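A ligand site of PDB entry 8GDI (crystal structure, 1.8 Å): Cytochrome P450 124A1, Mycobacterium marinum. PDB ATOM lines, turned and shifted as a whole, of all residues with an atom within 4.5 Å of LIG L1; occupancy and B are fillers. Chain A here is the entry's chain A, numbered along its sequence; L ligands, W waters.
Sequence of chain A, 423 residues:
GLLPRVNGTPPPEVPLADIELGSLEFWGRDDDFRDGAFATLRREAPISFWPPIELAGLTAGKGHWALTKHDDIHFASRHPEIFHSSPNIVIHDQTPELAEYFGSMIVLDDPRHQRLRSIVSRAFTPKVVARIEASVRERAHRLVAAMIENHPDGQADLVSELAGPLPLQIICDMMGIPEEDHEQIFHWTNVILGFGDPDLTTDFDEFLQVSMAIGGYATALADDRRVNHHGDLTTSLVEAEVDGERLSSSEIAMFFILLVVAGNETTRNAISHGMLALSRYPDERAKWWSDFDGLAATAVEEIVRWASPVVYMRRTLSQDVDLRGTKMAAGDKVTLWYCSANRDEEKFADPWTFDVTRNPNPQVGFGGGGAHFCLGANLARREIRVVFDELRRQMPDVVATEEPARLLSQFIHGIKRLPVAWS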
ATOM      1  N   ALA A  56      32.773 -31.968 -26.152  1.00  0.00           N
ATOM      2  CA  ALA A  56      32.195 -31.684 -27.473  1.00  0.00           C
ATOM      3  C   ALA A  56      33.275 -31.329 -28.499  1.00  0.00           C
ATOM      4  O   ALA A  56      33.070 -30.514 -29.403  1.00  0.00           O
ATOM      5  CB  ALA A  56      31.135 -30.580 -27.386  1.00  0.00           C
ATOM      6  N   ASN A  88      32.846 -15.791 -32.059  1.00  0.00           N
ATOM      7  CA  ASN A  88      32.575 -16.323 -30.718  1.00  0.00           C
ATOM      8  C   ASN A  88      33.696 -15.927 -29.777  1.00  0.00           C
ATOM      9  O   ASN A  88      34.813 -15.625 -30.198  1.00  0.00           O
ATOM     10  CB  ASN A  88      32.418 -17.854 -30.753  1.00  0.00           C
ATOM     11  CG  ASN A  88      31.565 -18.386 -29.605  1.00  0.00           C
ATOM     12  OD1 ASN A  88      30.980 -17.624 -28.822  1.00  0.00           O
ATOM     13  ND2 ASN A  88      31.507 -19.707 -29.511  1.00  0.00           N
ATOM     14  N   ILE A  89      33.368 -15.911 -28.491  1.00  0.00           N
ATOM     15  CA  ILE A  89      34.321 -15.534 -27.450  1.00  0.00           C
ATOM     16  C   ILE A  89      34.724 -16.707 -26.561  1.00  0.00           C
ATOM     17  O   ILE A  89      35.465 -16.495 -25.590  1.00  0.00           O
ATOM     18  CB  ILE A  89      33.776 -14.378 -26.587  1.00  0.00           C
ATOM     19  CG1 ILE A  89      32.299 -14.614 -26.271  1.00  0.00           C
ATOM     20  CG2 ILE A  89      33.908 -13.071 -27.364  1.00  0.00           C
ATOM     21  CD1 ILE A  89      32.069 -15.436 -25.005  1.00  0.00           C
ATOM     22  N   VAL A  90      34.279 -17.927 -26.846  1.00  0.00           N
ATOM     23  CA  VAL A  90      34.868 -19.119 -26.272  1.00  0.00           C
ATOM     24  C   VAL A  90      35.599 -19.832 -27.415  1.00  0.00           C
ATOM     25  O   VAL A  90      35.451 -19.474 -28.581  1.00  0.00           O
ATOM     26  CB  VAL A  90      33.840 -20.058 -25.600  1.00  0.00           C
ATOM     27  CG1 VAL A  90      33.336 -19.436 -24.280  1.00  0.00           C
ATOM     28  CG2 VAL A  90      32.717 -20.418 -26.547  1.00  0.00           C
ATOM     29  N   HIS A  92      35.225 -22.959 -28.504  1.00  0.00           N
ATOM     30  CA  HIS A  92      34.359 -23.797 -29.339  1.00  0.00           C
ATOM     31  C   HIS A  92      33.661 -22.953 -30.406  1.00  0.00           C
ATOM     32  O   HIS A  92      33.151 -21.864 -30.125  1.00  0.00           O
ATOM     33  CB  HIS A  92      33.317 -24.492 -28.469  1.00  0.00           C
ATOM     34  CG  HIS A  92      32.716 -25.728 -29.083  1.00  0.00           C
ATOM     35  ND1 HIS A  92      31.800 -25.669 -30.115  1.00  0.00           N
ATOM     36  CD2 HIS A  92      32.858 -27.035 -28.784  1.00  0.00           C
ATOM     37  CE1 HIS A  92      31.437 -26.908 -30.442  1.00  0.00           C
ATOM     38  NE2 HIS A  92      32.065 -27.751 -29.652  1.00  0.00           N
ATOM     39  N   GLN A  94      30.734 -21.574 -32.569  1.00  0.00           N
ATOM     40  CA  GLN A  94      29.300 -21.408 -32.303  1.00  0.00           C
ATOM     41  C   GLN A  94      28.516 -21.993 -33.455  1.00  0.00           C
ATOM     42  O   GLN A  94      28.239 -21.315 -34.454  1.00  0.00           O
ATOM     43  CB  GLN A  94      28.924 -19.943 -32.087  1.00  0.00           C
ATOM     44  CG  GLN A  94      27.766 -19.807 -31.115  1.00  0.00           C
ATOM     45  CD  GLN A  94      27.429 -18.370 -30.805  1.00  0.00           C
ATOM     46  OE1 GLN A  94      26.806 -17.678 -31.605  1.00  0.00           O
ATOM     47  NE2 GLN A  94      27.865 -17.916 -29.629  1.00  0.00           N
ATOM     48  N   LEU A  98      23.719 -23.575 -31.416  1.00  0.00           N
ATOM     49  CA  LEU A  98      24.127 -22.725 -30.305  1.00  0.00           C
ATOM     50  C   LEU A  98      23.886 -21.261 -30.621  1.00  0.00           C
ATOM     51  O   LEU A  98      23.533 -20.484 -29.729  1.00  0.00           O
ATOM     52  CB  LEU A  98      25.602 -22.945 -29.976  1.00  0.00           C
ATOM     53  CG  LEU A  98      25.948 -24.245 -29.253  1.00  0.00           C
ATOM     54  CD1 LEU A  98      27.444 -24.588 -29.417  1.00  0.00           C
ATOM     55  CD2 LEU A  98      25.554 -24.184 -27.771  1.00  0.00           C
ATOM     56  N   PHE A 102      22.870 -17.938 -28.281  1.00  0.00           N
ATOM     57  CA  PHE A 102      24.034 -17.252 -27.741  1.00  0.00           C
ATOM     58  C   PHE A 102      24.657 -16.232 -28.699  1.00  0.00           C
ATOM     59  O   PHE A 102      25.698 -15.647 -28.367  1.00  0.00           O
ATOM     60  CB  PHE A 102      25.050 -18.292 -27.282  1.00  0.00           C
ATOM     61  CG  PHE A 102      24.501 -19.211 -26.222  1.00  0.00           C
ATOM     62  CD1 PHE A 102      24.114 -18.715 -24.991  1.00  0.00           C
ATOM     63  CD2 PHE A 102      24.329 -20.581 -26.479  1.00  0.00           C
ATOM     64  CE1 PHE A 102      23.596 -19.541 -24.019  1.00  0.00           C
ATOM     65  CE2 PHE A 102      23.806 -21.417 -25.508  1.00  0.00           C
ATOM     66  CZ  PHE A 102      23.429 -20.903 -24.275  1.00  0.00           C
ATOM     67  N   ILE A 106      27.739  -9.946 -27.300  1.00  0.00           N
ATOM     68  CA  ILE A 106      29.101 -10.260 -26.872  1.00  0.00           C
ATOM     69  C   ILE A 106      29.899 -10.932 -27.974  1.00  0.00           C
ATOM     70  O   ILE A 106      31.138 -10.878 -27.924  1.00  0.00           O
ATOM     71  CB  ILE A 106      29.099 -11.127 -25.586  1.00  0.00           C
ATOM     72  CG1 ILE A 106      30.446 -10.931 -24.844  1.00  0.00           C
ATOM     73  CG2 ILE A 106      28.764 -12.610 -25.901  1.00  0.00           C
ATOM     74  CD1 ILE A 106      30.526 -11.589 -23.448  1.00  0.00           C
ATOM     75  N   ILE A 192      24.088 -23.753 -18.042  1.00  0.00           N
ATOM     76  CA  ILE A 192      24.614 -23.129 -19.254  1.00  0.00           C
ATOM     77  C   ILE A 192      26.103 -22.840 -19.129  1.00  0.00           C
ATOM     78  O   ILE A 192      26.852 -22.958 -20.110  1.00  0.00           O
ATOM     79  CB  ILE A 192      23.807 -21.869 -19.598  1.00  0.00           C
ATOM     80  CG1 ILE A 192      22.422 -22.252 -20.146  1.00  0.00           C
ATOM     81  CG2 ILE A 192      24.563 -21.008 -20.613  1.00  0.00           C
ATOM     82  CD1 ILE A 192      21.468 -21.068 -20.212  1.00  0.00           C
ATOM     83  N   LEU A 193      26.571 -22.463 -17.930  1.00  0.00           N
ATOM     84  CA  LEU A 193      28.007 -22.275 -17.736  1.00  0.00           C
ATOM     85  C   LEU A 193      28.599 -23.346 -16.831  1.00  0.00           C
ATOM     86  O   LEU A 193      29.562 -23.089 -16.094  1.00  0.00           O
ATOM     87  CB  LEU A 193      28.317 -20.875 -17.203  1.00  0.00           C
ATOM     88  CG  LEU A 193      28.265 -19.811 -18.288  1.00  0.00           C
ATOM     89  CD1 LEU A 193      28.703 -18.470 -17.729  1.00  0.00           C
ATOM     90  CD2 LEU A 193      29.196 -20.198 -19.431  1.00  0.00           C
ATOM     91  N   PHE A 195      28.702 -26.765 -18.397  1.00  0.00           N
ATOM     92  CA  PHE A 195      28.741 -27.955 -19.257  1.00  0.00           C
ATOM     93  C   PHE A 195      30.086 -28.648 -19.129  1.00  0.00           C
ATOM     94  O   PHE A 195      31.135 -27.995 -19.159  1.00  0.00           O
ATOM     95  CB  PHE A 195      28.457 -27.593 -20.713  1.00  0.00           C
ATOM     96  CG  PHE A 195      28.485 -28.771 -21.643  1.00  0.00           C
ATOM     97  CD1 PHE A 195      27.524 -29.786 -21.530  1.00  0.00           C
ATOM     98  CD2 PHE A 195      29.460 -28.877 -22.614  1.00  0.00           C
ATOM     99  CE1 PHE A 195      27.550 -30.900 -22.404  1.00  0.00           C
ATOM    100  CE2 PHE A 195      29.493 -29.972 -23.478  1.00  0.00           C
ATOM    101  CZ  PHE A 195      28.540 -30.991 -23.361  1.00  0.00           C
ATOM    102  N   PHE A 204      24.880 -33.076 -23.667  1.00  0.00           N
ATOM    103  CA  PHE A 204      24.595 -31.873 -24.451  1.00  0.00           C
ATOM    104  C   PHE A 204      23.107 -31.727 -24.764  1.00  0.00           C
ATOM    105  O   PHE A 204      22.642 -30.607 -24.946  1.00  0.00           O
ATOM    106  CB  PHE A 204      25.417 -31.850 -25.735  1.00  0.00           C
ATOM    107  CG  PHE A 204      25.422 -30.492 -26.417  1.00  0.00           C
ATOM    108  CD1 PHE A 204      25.910 -29.381 -25.743  1.00  0.00           C
ATOM    109  CD2 PHE A 204      24.911 -30.328 -27.685  1.00  0.00           C
ATOM    110  CE1 PHE A 204      25.906 -28.126 -26.349  1.00  0.00           C
ATOM    111  CE2 PHE A 204      24.898 -29.092 -28.292  1.00  0.00           C
ATOM    112  CZ  PHE A 204      25.398 -27.986 -27.623  1.00  0.00           C
ATOM    113  N   PHE A 207      21.808 -29.783 -21.891  1.00  0.00           N
ATOM    114  CA  PHE A 207      22.210 -28.397 -22.163  1.00  0.00           C
ATOM    115  C   PHE A 207      21.223 -27.724 -23.112  1.00  0.00           C
ATOM    116  O   PHE A 207      20.766 -26.594 -22.871  1.00  0.00           O
ATOM    117  CB  PHE A 207      23.619 -28.367 -22.747  1.00  0.00           C
ATOM    118  CG  PHE A 207      24.150 -26.971 -23.014  1.00  0.00           C
ATOM    119  CD1 PHE A 207      23.832 -26.303 -24.179  1.00  0.00           C
ATOM    120  CD2 PHE A 207      24.995 -26.344 -22.103  1.00  0.00           C
ATOM    121  CE1 PHE A 207      24.311 -25.018 -24.419  1.00  0.00           C
ATOM    122  CE2 PHE A 207      25.481 -25.073 -22.349  1.00  0.00           C
ATOM    123  CZ  PHE A 207      25.135 -24.403 -23.504  1.00  0.00           C
ATOM    124  N   LEU A 258      22.053 -13.352 -22.211  1.00  0.00           N
ATOM    125  CA  LEU A 258      23.371 -12.812 -21.916  1.00  0.00           C
ATOM    126  C   LEU A 258      23.396 -12.173 -20.535  1.00  0.00           C
ATOM    127  O   LEU A 258      24.265 -12.465 -19.716  1.00  0.00           O
ATOM    128  CB  LEU A 258      23.787 -11.797 -22.997  1.00  0.00           C
ATOM    129  CG  LEU A 258      25.055 -10.989 -22.715  1.00  0.00           C
ATOM    130  CD1 LEU A 258      26.254 -11.912 -22.558  1.00  0.00           C
ATOM    131  CD2 LEU A 258      25.311  -9.909 -23.801  1.00  0.00           C
ATOM    132  N   VAL A 261      22.839 -14.745 -17.523  1.00  0.00           N
ATOM    133  CA  VAL A 261      23.956 -15.671 -17.353  1.00  0.00           C
ATOM    134  C   VAL A 261      25.162 -14.929 -16.805  1.00  0.00           C
ATOM    135  O   VAL A 261      25.847 -15.401 -15.893  1.00  0.00           O
ATOM    136  CB  VAL A 261      24.291 -16.361 -18.686  1.00  0.00           C
ATOM    137  CG1 VAL A 261      25.658 -17.006 -18.599  1.00  0.00           C
ATOM    138  CG2 VAL A 261      23.212 -17.390 -19.059  1.00  0.00           C
ATOM    139  N   ALA A 262      25.458 -13.749 -17.372  1.00  0.00           N
ATOM    140  CA  ALA A 262      26.605 -12.980 -16.904  1.00  0.00           C
ATOM    141  C   ALA A 262      26.418 -12.515 -15.473  1.00  0.00           C
ATOM    142  O   ALA A 262      27.358 -12.547 -14.673  1.00  0.00           O
ATOM    143  CB  ALA A 262      26.832 -11.782 -17.835  1.00  0.00           C
ATOM    144  N   THR A 266      29.359 -15.029 -12.230  1.00  0.00           N
ATOM    145  CA  THR A 266      30.609 -14.263 -12.177  1.00  0.00           C
ATOM    146  C   THR A 266      30.851 -13.756 -10.759  1.00  0.00           C
ATOM    147  O   THR A 266      31.741 -14.244 -10.067  1.00  0.00           O
ATOM    148  CB  THR A 266      30.563 -13.074 -13.146  1.00  0.00           C
ATOM    149  OG1 THR A 266      29.375 -12.322 -12.898  1.00  0.00           O
ATOM    150  CG2 THR A 266      30.562 -13.558 -14.626  1.00  0.00           C
ATOM    151  N   VAL A 310      36.359 -14.855 -14.651  1.00  0.00           N
ATOM    152  CA  VAL A 310      36.359 -15.254 -16.055  1.00  0.00           C
ATOM    153  C   VAL A 310      37.800 -15.566 -16.407  1.00  0.00           C
ATOM    154  O   VAL A 310      38.679 -14.707 -16.271  1.00  0.00           O
ATOM    155  CB  VAL A 310      35.798 -14.155 -16.963  1.00  0.00           C
ATOM    156  CG1 VAL A 310      35.992 -14.540 -18.446  1.00  0.00           C
ATOM    157  CG2 VAL A 310      34.329 -13.884 -16.627  1.00  0.00           C
ATOM    158  N   MET A 313      38.861 -15.089 -22.590  1.00  0.00           N
ATOM    159  CA  MET A 313      37.860 -14.722 -23.622  1.00  0.00           C
ATOM    160  C   MET A 313      38.566 -14.845 -24.997  1.00  0.00           C
ATOM    161  O   MET A 313      39.783 -14.674 -24.993  1.00  0.00           O
ATOM    162  CB  MET A 313      37.302 -13.316 -23.436  1.00  0.00           C
ATOM    163  CG  MET A 313      36.247 -13.185 -22.370  1.00  0.00           C
ATOM    164  SD  MET A 313      34.607 -13.610 -22.956  1.00  0.00           S
ATOM    165  CE  MET A 313      33.661 -13.318 -21.470  1.00  0.00           C
ATOM    166  N   PHE A 411      36.657 -22.002 -18.765  1.00  0.00           N
ATOM    167  CA  PHE A 411      36.174 -20.640 -19.009  1.00  0.00           C
ATOM    168  C   PHE A 411      35.847 -19.871 -17.728  1.00  0.00           C
ATOM    169  O   PHE A 411      36.068 -18.649 -17.680  1.00  0.00           O
ATOM    170  CB  PHE A 411      34.937 -20.735 -19.917  1.00  0.00           C
ATOM    171  CG  PHE A 411      34.337 -19.410 -20.331  1.00  0.00           C
ATOM    172  CD1 PHE A 411      35.112 -18.379 -20.853  1.00  0.00           C
ATOM    173  CD2 PHE A 411      32.963 -19.220 -20.217  1.00  0.00           C
ATOM    174  CE1 PHE A 411      34.529 -17.180 -21.243  1.00  0.00           C
ATOM    175  CE2 PHE A 411      32.366 -18.037 -20.599  1.00  0.00           C
ATOM    176  CZ  PHE A 411      33.151 -17.001 -21.108  1.00  0.00           C
ATOM    177  N   ILE A 412      35.362 -20.561 -16.686  1.00  0.00           N
ATOM    178  CA  ILE A 412      34.799 -19.944 -15.486  1.00  0.00           C
ATOM    179  C   ILE A 412      35.527 -20.529 -14.271  1.00  0.00           C
ATOM    180  O   ILE A 412      35.586 -21.747 -14.113  1.00  0.00           O
ATOM    181  CB  ILE A 412      33.285 -20.214 -15.374  1.00  0.00           C
ATOM    182  CG1 ILE A 412      32.520 -19.599 -16.554  1.00  0.00           C
ATOM    183  CG2 ILE A 412      32.724 -19.793 -13.995  1.00  0.00           C
ATOM    184  CD1 ILE A 412      32.375 -18.079 -16.472  1.00  0.00           C
HETATM  185  C1  LIG L   1      29.328 -23.095 -24.798  1.00  0.00           C
HETATM  186  C2  LIG L   1      28.163 -21.461 -23.213  1.00  0.00           C
HETATM  187  C3  LIG L   1      27.444 -20.128 -23.014  1.00  0.00           C
HETATM  188  C4  LIG L   1      28.213 -18.981 -23.674  1.00  0.00           C
HETATM  189  C5  LIG L   1      28.304 -19.309 -25.183  1.00  0.00           C
HETATM  190  C6  LIG L   1      28.819 -18.005 -25.800  1.00  0.00           C
HETATM  191  C7  LIG L   1      28.279 -16.889 -24.887  1.00  0.00           C
HETATM  192  C8  LIG L   1      27.502 -17.598 -23.749  1.00  0.00           C
HETATM  193  C9  LIG L   1      29.614 -18.829 -23.046  1.00  0.00           C
HETATM  194  C10 LIG L   1      28.442 -21.814 -24.678  1.00  0.00           C
HETATM  195  C11 LIG L   1      30.622 -22.970 -23.947  1.00  0.00           C
HETATM  196  C12 LIG L   1      28.504 -24.282 -24.283  1.00  0.00           C
HETATM  197  C13 LIG L   1      29.044 -25.666 -24.642  1.00  0.00           C
HETATM  198  C14 LIG L   1      29.255 -25.809 -26.129  1.00  0.00           C
HETATM  199  O1  LIG L   1      29.829 -27.092 -26.412  1.00  0.00           O
HETATM  200  C15 LIG L   1      30.209 -24.720 -26.591  1.00  0.00           C
HETATM  201  C16 LIG L   1      29.735 -23.337 -26.239  1.00  0.00           C
HETATM  202  C17 LIG L   1      29.703 -22.374 -27.172  1.00  0.00           C
HETATM  203  C18 LIG L   1      29.202 -21.027 -26.913  1.00  0.00           C
HETATM  204  O2  LIG L   1      28.944 -20.294 -27.859  1.00  0.00           O
HETATM  205  C19 LIG L   1      29.044 -20.625 -25.462  1.00  0.00           C
HETATM  206  C20 LIG L   1      27.294 -16.757 -22.475  1.00  0.00           C
HETATM  207  C21 LIG L   1      25.905 -16.148 -22.371  1.00  0.00           C
HETATM  208  C22 LIG L   1      28.370 -15.669 -22.263  1.00  0.00           C
HETATM  209  C23 LIG L   1      28.588 -15.288 -20.815  1.00  0.00           C
HETATM  210  C24 LIG L   1      29.628 -14.226 -20.613  1.00  0.00           C
HETATM  211  C25 LIG L   1      29.923 -13.863 -19.165  1.00  0.00           C
HETATM  212  C26 LIG L   1      30.615 -12.513 -19.061  1.00  0.00           C
HETATM  213  C27 LIG L   1      30.759 -14.925 -18.480  1.00  0.00           C
HETATM  214  C1  LG2 L   2      31.565  -8.839 -20.246  1.00  0.00           C
HETATM  215  C2  LG2 L   2      34.041 -10.309 -16.289  1.00  0.00           C
HETATM  216  C3  LG2 L   2      30.127  -9.435 -13.533  1.00  0.00           C
HETATM  217  C4  LG2 L   2      27.544  -8.361 -17.510  1.00  0.00           C
HETATM  218  C5  LG2 L   2      32.574  -9.298 -19.426  1.00  0.00           C
HETATM  219  C6  LG2 L   2      33.934  -9.618 -19.829  1.00  0.00           C
HETATM  220  C7  LG2 L   2      34.582 -10.039 -18.721  1.00  0.00           C
HETATM  221  C8  LG2 L   2      33.686  -9.966 -17.586  1.00  0.00           C
HETATM  222  C9  LG2 L   2      36.038 -10.521 -18.568  1.00  0.00           C
HETATM  223  C10 LG2 L   2      34.514  -9.510 -21.263  1.00  0.00           C
HETATM  224  C11 LG2 L   2      35.330  -8.205 -21.321  1.00  0.00           C
HETATM  225  C12 LG2 L   2      36.049  -8.008 -22.648  1.00  0.00           C
HETATM  226  O1  LG2 L   2      35.757  -8.760 -23.620  1.00  0.00           O
HETATM  227  O2  LG2 L   2      36.926  -7.098 -22.737  1.00  0.00           O
HETATM  228  C13 LG2 L   2      33.214 -10.170 -15.168  1.00  0.00           C
HETATM  229  C14 LG2 L   2      33.577 -10.354 -13.770  1.00  0.00           C
HETATM  230  C15 LG2 L   2      32.486 -10.113 -13.025  1.00  0.00           C
HETATM  231  C16 LG2 L   2      31.408  -9.759 -13.934  1.00  0.00           C
HETATM  232  C17 LG2 L   2      34.961 -10.767 -13.244  1.00  0.00           C
HETATM  233  C18 LG2 L   2      32.293 -10.154 -11.484  1.00  0.00           C
HETATM  234  C19 LG2 L   2      33.262  -9.982 -10.571  1.00  0.00           C
HETATM  235  C20 LG2 L   2      29.085  -9.083 -14.362  1.00  0.00           C
HETATM  236  C21 LG2 L   2      27.750  -8.779 -13.925  1.00  0.00           C
HETATM  237  C22 LG2 L   2      27.024  -8.489 -15.002  1.00  0.00           C
HETATM  238  C23 LG2 L   2      27.889  -8.576 -16.190  1.00  0.00           C
HETATM  239  C24 LG2 L   2      27.256  -8.799 -12.460  1.00  0.00           C
HETATM  240  C25 LG2 L   2      25.535  -8.108 -14.938  1.00  0.00           C
HETATM  241  C26 LG2 L   2      24.705  -8.267 -15.971  1.00  0.00           C
HETATM  242  C27 LG2 L   2      28.395  -8.413 -18.600  1.00  0.00           C
HETATM  243  C28 LG2 L   2      28.045  -8.169 -19.979  1.00  0.00           C
HETATM  244  C29 LG2 L   2      29.148  -8.291 -20.736  1.00  0.00           C
HETATM  245  C30 LG2 L   2      30.246  -8.631 -19.854  1.00  0.00           C
HETATM  246  C31 LG2 L   2      26.632  -7.821 -20.497  1.00  0.00           C
HETATM  247  C32 LG2 L   2      29.244  -8.117 -22.279  1.00  0.00           C
HETATM  248  C33 LG2 L   2      29.617  -6.654 -22.606  1.00  0.00           C
HETATM  249  C34 LG2 L   2      29.780  -6.384 -24.093  1.00  0.00           C
HETATM  250  O3  LG2 L   2      29.870  -7.342 -24.910  1.00  0.00           O
HETATM  251  O4  LG2 L   2      29.844  -5.182 -24.481  1.00  0.00           O
HETATM  252  N1  LG2 L   2      32.467  -9.521 -18.053  1.00  0.00           N
HETATM  253  N2  LG2 L   2      31.885  -9.809 -15.234  1.00  0.00           N
HETATM  254  N3  LG2 L   2      29.145  -8.948 -15.741  1.00  0.00           N
HETATM  255  N4  LG2 L   2      29.758  -8.688 -18.555  1.00  0.00           N
HETATM  256 FE1  LG2 L   2      30.894  -8.926 -16.851  1.00  0.00          FE
HETATM  257  O   HOH W   1      32.242 -27.699 -25.397  1.00  0.00           O
HETATM  258  O   HOH W   2      28.573 -28.492 -28.359  1.00  0.00           O
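The side-chain amide nitrogen of Asn 88 is in hydrogen-bond range of an oxygen (O2) of LIG L1, at 3.1 Å.
The side-chain amide nitrogen (NE2) of Gln 94 lies within hydrogen-bond range of an oxygen (O2) of LIG L1, 3.2 Å away.
The side-chain amide nitrogen (NE2) of Gln 94 sits at hydrogen-bond distance from the side-chain amide oxygen (OD1) of Asn 88, at 3.2 Å.
O of His 92 sits at hydrogen-bond distance from ND2 of Asn 88 (2.8 Å).
O of Phe 102 sits at hydrogen-bond distance from NE2 of Gln 94, at 3.4 Å.
NE2 of His 92 sits at hydrogen-bond distance from O of Ala 56 (3.0 Å).
OG1 of Thr 266 is in hydrogen-bond range of O of Ala 262 (2.7 Å).
CB of Ala 56 touches O1 of LIG L1, at 3.8 Å.
Val 90 touches LIG L1 (CG2 to C18, 3.6 Å).
His 92 touches LIG L1.
Leu 98 touches LIG L1.
Phe 102 touches LIG L1 (CD1 to C8, 3.8 Å).
Ile 106 touches LIG L1.
Ile 192 touches LIG L1.
Leu 193 touches LIG L1 (CD2 to C9, 3.9 Å).
CD2 of Phe 195 touches C13 of LIG L1, 3.8 Å away.
CZ of Phe 207 touches C12 of LIG L1, 3.5 Å away.
Val 261 touches LIG L1.
Ala 262 touches LIG L1.
CE of Met 313 touches C26 of LIG L1, at 3.97 Å.
Phe 411 touches LIG L1 (CE2 to C9, 3.8 Å).
Hydrophobic or aromatic side chains within 4 Å of LIG L1: Ala 56, Val 90, His 92, Leu 98, Phe 102, Ile 106, Ile 192, Leu 193, Phe 195, Phe 207, Val 261, Ala 262, Met 313 and Phe 411.
Within 4 Å of LIG L1: Ala 56, Asn 88, Val 90, His 92, Gln 94, Leu 98, Phe 102, Ile 106, Ile 192, Leu 193, Phe 195, Phe 207, Val 261, Ala 262, Met 313 and Phe 411.
The nearest printed residue that does not touch LIG L1 is Phe 204 (4.1 Å).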
